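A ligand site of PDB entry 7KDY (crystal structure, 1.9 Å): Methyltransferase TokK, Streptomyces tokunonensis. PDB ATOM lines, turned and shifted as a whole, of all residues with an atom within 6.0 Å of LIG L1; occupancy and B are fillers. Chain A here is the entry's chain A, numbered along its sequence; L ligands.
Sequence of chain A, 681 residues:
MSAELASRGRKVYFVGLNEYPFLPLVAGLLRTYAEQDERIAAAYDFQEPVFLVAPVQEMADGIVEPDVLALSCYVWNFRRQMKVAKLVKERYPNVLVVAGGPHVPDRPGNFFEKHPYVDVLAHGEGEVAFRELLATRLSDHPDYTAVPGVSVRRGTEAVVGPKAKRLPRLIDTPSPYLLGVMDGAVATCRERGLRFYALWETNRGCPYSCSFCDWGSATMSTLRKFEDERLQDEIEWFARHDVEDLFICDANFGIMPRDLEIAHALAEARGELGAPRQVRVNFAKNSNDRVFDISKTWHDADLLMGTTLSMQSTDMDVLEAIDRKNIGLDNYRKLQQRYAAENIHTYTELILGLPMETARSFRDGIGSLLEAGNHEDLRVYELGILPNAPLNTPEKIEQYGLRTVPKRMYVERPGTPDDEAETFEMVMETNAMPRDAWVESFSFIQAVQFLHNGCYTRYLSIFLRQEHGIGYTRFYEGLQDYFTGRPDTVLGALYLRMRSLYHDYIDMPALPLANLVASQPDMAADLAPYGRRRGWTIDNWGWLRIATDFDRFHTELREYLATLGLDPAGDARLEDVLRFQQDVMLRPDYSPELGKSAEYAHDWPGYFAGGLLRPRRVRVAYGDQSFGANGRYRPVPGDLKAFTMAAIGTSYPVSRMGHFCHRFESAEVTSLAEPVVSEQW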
ATOM      1  N   CYS A 206       2.098  19.024  -1.178  1.00  0.00           N
ATOM      2  CA  CYS A 206       1.653  19.780  -0.025  1.00  0.00           C
ATOM      3  C   CYS A 206       2.672  20.899   0.183  1.00  0.00           C
ATOM      4  O   CYS A 206       3.885  20.637   0.178  1.00  0.00           O
ATOM      5  CB  CYS A 206       1.534  18.939   1.238  1.00  0.00           C
ATOM      6  SG  CYS A 206       1.187  20.020   2.646  1.00  0.00           S
ATOM      7  N   PRO A 207       2.224  22.144   0.373  1.00  0.00           N
ATOM      8  CA  PRO A 207       3.190  23.234   0.525  1.00  0.00           C
ATOM      9  C   PRO A 207       3.853  23.281   1.883  1.00  0.00           C
ATOM     10  O   PRO A 207       4.829  24.028   2.037  1.00  0.00           O
ATOM     11  CB  PRO A 207       2.324  24.479   0.287  1.00  0.00           C
ATOM     12  CG  PRO A 207       0.946  24.075   0.700  1.00  0.00           C
ATOM     13  CD  PRO A 207       0.820  22.601   0.381  1.00  0.00           C
ATOM     14  N   TYR A 208       3.406  22.481   2.849  1.00  0.00           N
ATOM     15  CA  TYR A 208       3.846  22.576   4.236  1.00  0.00           C
ATOM     16  C   TYR A 208       4.954  21.546   4.507  1.00  0.00           C
ATOM     17  O   TYR A 208       5.441  20.882   3.588  1.00  0.00           O
ATOM     18  CB  TYR A 208       2.637  22.461   5.152  1.00  0.00           C
ATOM     19  CG  TYR A 208       1.552  23.427   4.725  1.00  0.00           C
ATOM     20  CD1 TYR A 208       1.775  24.809   4.748  1.00  0.00           C
ATOM     21  CD2 TYR A 208       0.325  22.979   4.266  1.00  0.00           C
ATOM     22  CE1 TYR A 208       0.802  25.706   4.344  1.00  0.00           C
ATOM     23  CE2 TYR A 208      -0.663  23.869   3.852  1.00  0.00           C
ATOM     24  CZ  TYR A 208      -0.418  25.220   3.898  1.00  0.00           C
ATOM     25  OH  TYR A 208      -1.398  26.090   3.483  1.00  0.00           O
ATOM     26  N   SER A 209       5.344  21.377   5.783  1.00  0.00           N
ATOM     27  CA  SER A 209       6.625  20.727   6.073  1.00  0.00           C
ATOM     28  C   SER A 209       6.592  19.851   7.319  1.00  0.00           C
ATOM     29  O   SER A 209       7.630  19.639   7.943  1.00  0.00           O
ATOM     30  CB  SER A 209       7.727  21.778   6.232  1.00  0.00           C
ATOM     31  OG  SER A 209       7.358  22.733   7.215  1.00  0.00           O
ATOM     32  N   CYS A 210       5.423  19.335   7.709  1.00  0.00           N
ATOM     33  CA  CYS A 210       5.347  18.511   8.912  1.00  0.00           C
ATOM     34  C   CYS A 210       6.327  17.329   8.826  1.00  0.00           C
ATOM     35  O   CYS A 210       6.280  16.554   7.877  1.00  0.00           O
ATOM     36  CB  CYS A 210       3.919  18.015   9.123  1.00  0.00           C
ATOM     37  SG  CYS A 210       2.747  19.375   9.165  1.00  0.00           S
ATOM     38  N   PHE A 212       6.863  14.492  10.283  1.00  0.00           N
ATOM     39  CA  PHE A 212       6.426  13.102  10.309  1.00  0.00           C
ATOM     40  C   PHE A 212       5.831  12.629   8.991  1.00  0.00           C
ATOM     41  O   PHE A 212       5.682  11.415   8.804  1.00  0.00           O
ATOM     42  CB  PHE A 212       5.391  12.894  11.424  1.00  0.00           C
ATOM     43  CG  PHE A 212       4.165  13.769  11.282  1.00  0.00           C
ATOM     44  CD1 PHE A 212       3.169  13.461  10.364  1.00  0.00           C
ATOM     45  CD2 PHE A 212       4.021  14.905  12.068  1.00  0.00           C
ATOM     46  CE1 PHE A 212       2.055  14.277  10.217  1.00  0.00           C
ATOM     47  CE2 PHE A 212       2.904  15.714  11.933  1.00  0.00           C
ATOM     48  CZ  PHE A 212       1.923  15.398  11.015  1.00  0.00           C
ATOM     49  N   CYS A 213       5.505  13.536   8.083  1.00  0.00           N
ATOM     50  CA  CYS A 213       4.655  13.245   6.939  1.00  0.00           C
ATOM     51  C   CYS A 213       5.462  13.023   5.665  1.00  0.00           C
ATOM     52  O   CYS A 213       6.554  13.552   5.492  1.00  0.00           O
ATOM     53  CB  CYS A 213       3.657  14.388   6.719  1.00  0.00           C
ATOM     54  SG  CYS A 213       2.370  14.009   5.534  1.00  0.00           S
ATOM     55  N   ASP A 214       4.887  12.237   4.752  1.00  0.00           N
ATOM     56  CA  ASP A 214       5.474  12.015   3.433  1.00  0.00           C
ATOM     57  C   ASP A 214       4.383  12.016   2.371  1.00  0.00           C
ATOM     58  O   ASP A 214       4.418  11.222   1.422  1.00  0.00           O
ATOM     59  CB  ASP A 214       6.280  10.716   3.401  1.00  0.00           C
ATOM     60  CG  ASP A 214       7.192  10.623   2.196  1.00  0.00           C
ATOM     61  OD1 ASP A 214       7.508  11.690   1.610  1.00  0.00           O
ATOM     62  OD2 ASP A 214       7.589   9.494   1.816  1.00  0.00           O
ATOM     63  N   TRP A 215       3.405  12.908   2.517  1.00  0.00           N
ATOM     64  CA  TRP A 215       2.205  12.911   1.689  1.00  0.00           C
ATOM     65  C   TRP A 215       2.542  12.962   0.198  1.00  0.00           C
ATOM     66  O   TRP A 215       3.113  13.948  -0.285  1.00  0.00           O
ATOM     67  CB  TRP A 215       1.328  14.107   2.059  1.00  0.00           C
ATOM     68  CG  TRP A 215      -0.104  13.905   1.693  1.00  0.00           C
ATOM     69  CD1 TRP A 215      -0.753  14.349   0.578  1.00  0.00           C
ATOM     70  CD2 TRP A 215      -1.081  13.168   2.452  1.00  0.00           C
ATOM     71  NE1 TRP A 215      -2.065  13.963   0.595  1.00  0.00           N
ATOM     72  CE2 TRP A 215      -2.300  13.230   1.735  1.00  0.00           C
ATOM     73  CE3 TRP A 215      -1.037  12.474   3.659  1.00  0.00           C
ATOM     74  CZ2 TRP A 215      -3.460  12.611   2.195  1.00  0.00           C
ATOM     75  CZ3 TRP A 215      -2.191  11.852   4.110  1.00  0.00           C
ATOM     76  CH2 TRP A 215      -3.385  11.936   3.381  1.00  0.00           C
ATOM     77  N   THR A 219       5.794  16.477   0.071  1.00  0.00           N
ATOM     78  CA  THR A 219       5.649  17.606   0.984  1.00  0.00           C
ATOM     79  C   THR A 219       6.684  18.676   0.638  1.00  0.00           C
ATOM     80  O   THR A 219       7.584  18.457  -0.168  1.00  0.00           O
ATOM     81  CB  THR A 219       5.803  17.159   2.435  1.00  0.00           C
ATOM     82  OG1 THR A 219       7.132  16.657   2.635  1.00  0.00           O
ATOM     83  CG2 THR A 219       4.784  16.057   2.776  1.00  0.00           C
ATOM     84  N   ALA A 251      -3.760  16.751  -0.467  1.00  0.00           N
ATOM     85  CA  ALA A 251      -3.292  17.021   0.884  1.00  0.00           C
ATOM     86  C   ALA A 251      -4.123  18.085   1.583  1.00  0.00           C
ATOM     87  O   ALA A 251      -4.320  18.013   2.803  1.00  0.00           O
ATOM     88  CB  ALA A 251      -1.828  17.458   0.851  1.00  0.00           C
ATOM     89  N   ASN A 252      -4.634  19.084   0.833  1.00  0.00           N
ATOM     90  CA  ASN A 252      -5.269  20.255   1.408  1.00  0.00           C
ATOM     91  C   ASN A 252      -6.481  20.668   0.560  1.00  0.00           C
ATOM     92  O   ASN A 252      -6.486  21.732  -0.068  1.00  0.00           O
ATOM     93  CB  ASN A 252      -4.286  21.424   1.503  1.00  0.00           C
ATOM     94  CG  ASN A 252      -3.161  21.160   2.478  1.00  0.00           C
ATOM     95  OD1 ASN A 252      -3.341  21.281   3.688  1.00  0.00           O
ATOM     96  ND2 ASN A 252      -1.991  20.787   1.954  1.00  0.00           N
ATOM     97  N   LYS A 285      -5.071  22.487   5.778  1.00  0.00           N
ATOM     98  CA  LYS A 285      -4.586  22.790   7.121  1.00  0.00           C
ATOM     99  C   LYS A 285      -5.013  24.175   7.567  1.00  0.00           C
ATOM    100  O   LYS A 285      -5.557  24.355   8.664  1.00  0.00           O
ATOM    101  CB  LYS A 285      -3.067  22.666   7.177  1.00  0.00           C
ATOM    102  CG  LYS A 285      -2.492  22.906   8.574  1.00  0.00           C
ATOM    103  CD  LYS A 285      -1.027  22.522   8.680  1.00  0.00           C
ATOM    104  CE  LYS A 285      -0.155  23.467   7.858  1.00  0.00           C
ATOM    105  NZ  LYS A 285      -0.242  24.858   8.372  1.00  0.00           N
ATOM    106  N   GLN A 312      -2.557  17.351  15.051  1.00  0.00           N
ATOM    107  CA  GLN A 312      -1.456  16.446  15.374  1.00  0.00           C
ATOM    108  C   GLN A 312      -1.029  16.619  16.832  1.00  0.00           C
ATOM    109  O   GLN A 312      -0.941  15.648  17.586  1.00  0.00           O
ATOM    110  CB  GLN A 312      -0.261  16.645  14.427  1.00  0.00           C
ATOM    111  CG  GLN A 312      -0.631  17.003  12.980  1.00  0.00           C
ATOM    112  CD  GLN A 312      -1.549  15.988  12.304  1.00  0.00           C
ATOM    113  OE1 GLN A 312      -1.878  14.945  12.875  1.00  0.00           O
ATOM    114  NE2 GLN A 312      -1.927  16.281  11.068  1.00  0.00           N
ATOM    115  N   ARG A 324       5.404  22.384  12.288  1.00  0.00           N
ATOM    116  CA  ARG A 324       3.993  22.561  11.946  1.00  0.00           C
ATOM    117  C   ARG A 324       3.432  23.758  12.706  1.00  0.00           C
ATOM    118  O   ARG A 324       3.663  23.891  13.907  1.00  0.00           O
ATOM    119  CB  ARG A 324       3.170  21.320  12.260  1.00  0.00           C
ATOM    120  CG  ARG A 324       1.684  21.479  11.930  1.00  0.00           C
ATOM    121  CD  ARG A 324       0.907  20.217  12.283  1.00  0.00           C
ATOM    122  NE  ARG A 324      -0.531  20.402  12.119  1.00  0.00           N
ATOM    123  CZ  ARG A 324      -1.227  19.987  11.067  1.00  0.00           C
ATOM    124  NH1 ARG A 324      -0.628  19.347  10.072  1.00  0.00           N
ATOM    125  NH2 ARG A 324      -2.535  20.202  11.015  1.00  0.00           N
HETATM  126 FE1  LIG L   1       1.444  18.487   7.213  1.00  0.00          FE
HETATM  127 FE2  LIG L   1       1.008  18.631   4.590  1.00  0.00          FE
HETATM  128 FE3  LIG L   1      -1.011  17.734   6.246  1.00  0.00          FE
HETATM  129 FE4  LIG L   1       1.256  16.237   5.770  1.00  0.00          FE
HETATM  130  S1  LIG L   1      -0.294  16.816   4.261  1.00  0.00           S
HETATM  131  S2  LIG L   1       0.272  16.624   7.781  1.00  0.00           S
HETATM  132  S3  LIG L   1       2.844  17.834   5.580  1.00  0.00           S
HETATM  133  S4  LIG L   1      -0.021  19.830   6.220  1.00  0.00           S
HETATM  134  N1  LG2 L   2      -2.991  18.807   5.312  1.00  0.00           N
HETATM  135  C1  LG2 L   2      -4.058  18.855   6.316  1.00  0.00           C
HETATM  136  C2  LG2 L   2      -3.496  19.021   7.722  1.00  0.00           C
HETATM  137  O1  LG2 L   2      -2.376  18.613   8.038  1.00  0.00           O
HETATM  138  C3  LG2 L   2      -4.929  17.602   6.234  1.00  0.00           C
HETATM  139  C4  LG2 L   2      -4.416  16.398   7.011  1.00  0.00           C
HETATM  140  S1  LG2 L   2      -2.879  15.712   6.376  1.00  0.00           S
HETATM  141  C5  LG2 L   2      -3.351  15.293   4.707  1.00  0.00           C
HETATM  142  O2  LG2 L   2      -4.164  19.575   8.601  1.00  0.00           O
HETATM  143  N1  LG3 L   3       2.242   8.555  11.551  1.00  0.00           N
HETATM  144  C1  LG3 L   3       0.965   8.606  11.951  1.00  0.00           C
HETATM  145  N2  LG3 L   3      -0.032   9.350  11.465  1.00  0.00           N
HETATM  146  C2  LG3 L   3       0.369  10.095  10.429  1.00  0.00           C
HETATM  147  N3  LG3 L   3      -0.374  10.987   9.700  1.00  0.00           N
HETATM  148  C3  LG3 L   3       0.468  11.497   8.762  1.00  0.00           C
HETATM  149  N4  LG3 L   3       1.701  11.029   8.835  1.00  0.00           N
HETATM  150  C4  LG3 L   3       1.639  10.136   9.900  1.00  0.00           C
HETATM  151  C5  LG3 L   3       2.625   9.327  10.507  1.00  0.00           C
HETATM  152  N5  LG3 L   3       3.898   9.332  10.115  1.00  0.00           N
HETATM  153  C6  LG3 L   3      -1.771  11.347   9.938  1.00  0.00           C
HETATM  154  C7  LG3 L   3      -1.970  12.795  10.396  1.00  0.00           C
HETATM  155  C8  LG3 L   3      -2.676  13.433   9.191  1.00  0.00           C
HETATM  156  C9  LG3 L   3      -3.442  12.254   8.614  1.00  0.00           C
HETATM  157  C10 LG3 L   3      -3.864  12.389   7.172  1.00  0.00           C
HETATM  158  O1  LG3 L   3      -2.505  11.163   8.739  1.00  0.00           O
HETATM  159  O2  LG3 L   3      -2.802  12.789  11.556  1.00  0.00           O
HETATM  160  O3  LG3 L   3      -3.588  14.462   9.563  1.00  0.00           O
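NH1 of Arg 324 lies close to S2 of LIG L1.
FE1 of LIG L1 is bound by SG of Cys 210 (2.5 Å).
The side-chain amide oxygen (OE1) of Gln 312 is in hydrogen-bond range of an oxygen (O2) of LG3 L3 (2.7 Å).
An iron atom (FE4) of LIG L1 is bound by the side-chain sulfur (SG) of Cys 213.
The backbone carbonyl oxygen (O) of Ala 251 sits close to a nitrogen (N1) of LG2 L2, 2.9 Å away.
NH2 of Arg 324 lies within salt-bridge range of O2 of LG2 L2.
The side-chain amide oxygen (OD1) of Asn 252 lies close to a nitrogen (N1) of LG2 L2 (3.0 Å).
A nitrogen (N5) of LG3 L3 sits at hydrogen-bond distance from the backbone carbonyl oxygen (O) of Phe 212, 3.0 Å away.
The side-chain sulfur (SG) of Cys 206 is bound to an iron atom (FE2) of LIG L1.
The backbone NH of Cys 210 sits close to a sulfur (S3) of LIG L1.
Tyr 208 touches LIG L1.
CE1 of Phe 212 touches S2 of LIG L1 (3.8 Å).
Trp 215 touches LIG L1.
Thr 219 touches LIG L1.
Ala 251 touches LIG L1 (CB to S1, 3.8 Å).
Lys 285 touches LIG L1.
Gln 312 touches LIG L1.
Of the 15 residues printed, 11 come within 4 Å of LIG L1.
Along chain A the residues within 4 Å of LIG L1 span positions 206 to 324.
The nearest printed residue that does not touch LIG L1 is Ser 209 (4.3 Å).
The side-chain sulfur (SG) of Cys 213 sits close to the backbone NH (N) of Trp 215, at 3.4 Å.
The side-chain sulfur (SG) of Cys 206 lies close to the backbone NH (N) of Tyr 208, at 3.3 Å.
NH1 of Arg 324 lies close to SG of Cys 210, 3.5 Å away.
OD1 of Asn 252 lies within hydrogen-bond range of N of Lys 285 (3.0 Å).
The side-chain sulfur (SG) of Cys 206 lies close to the side-chain amide nitrogen (ND2) of Asn 252.
NH1 of Arg 324 lies close to NE2 of Gln 312 (3.5 Å).
FE3 of LIG L1 is bound by O1 of LG2 L2 (2.4 Å).
S1 of LG2 L2 lies close to O3 of LG3 L3 (3.5 Å).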
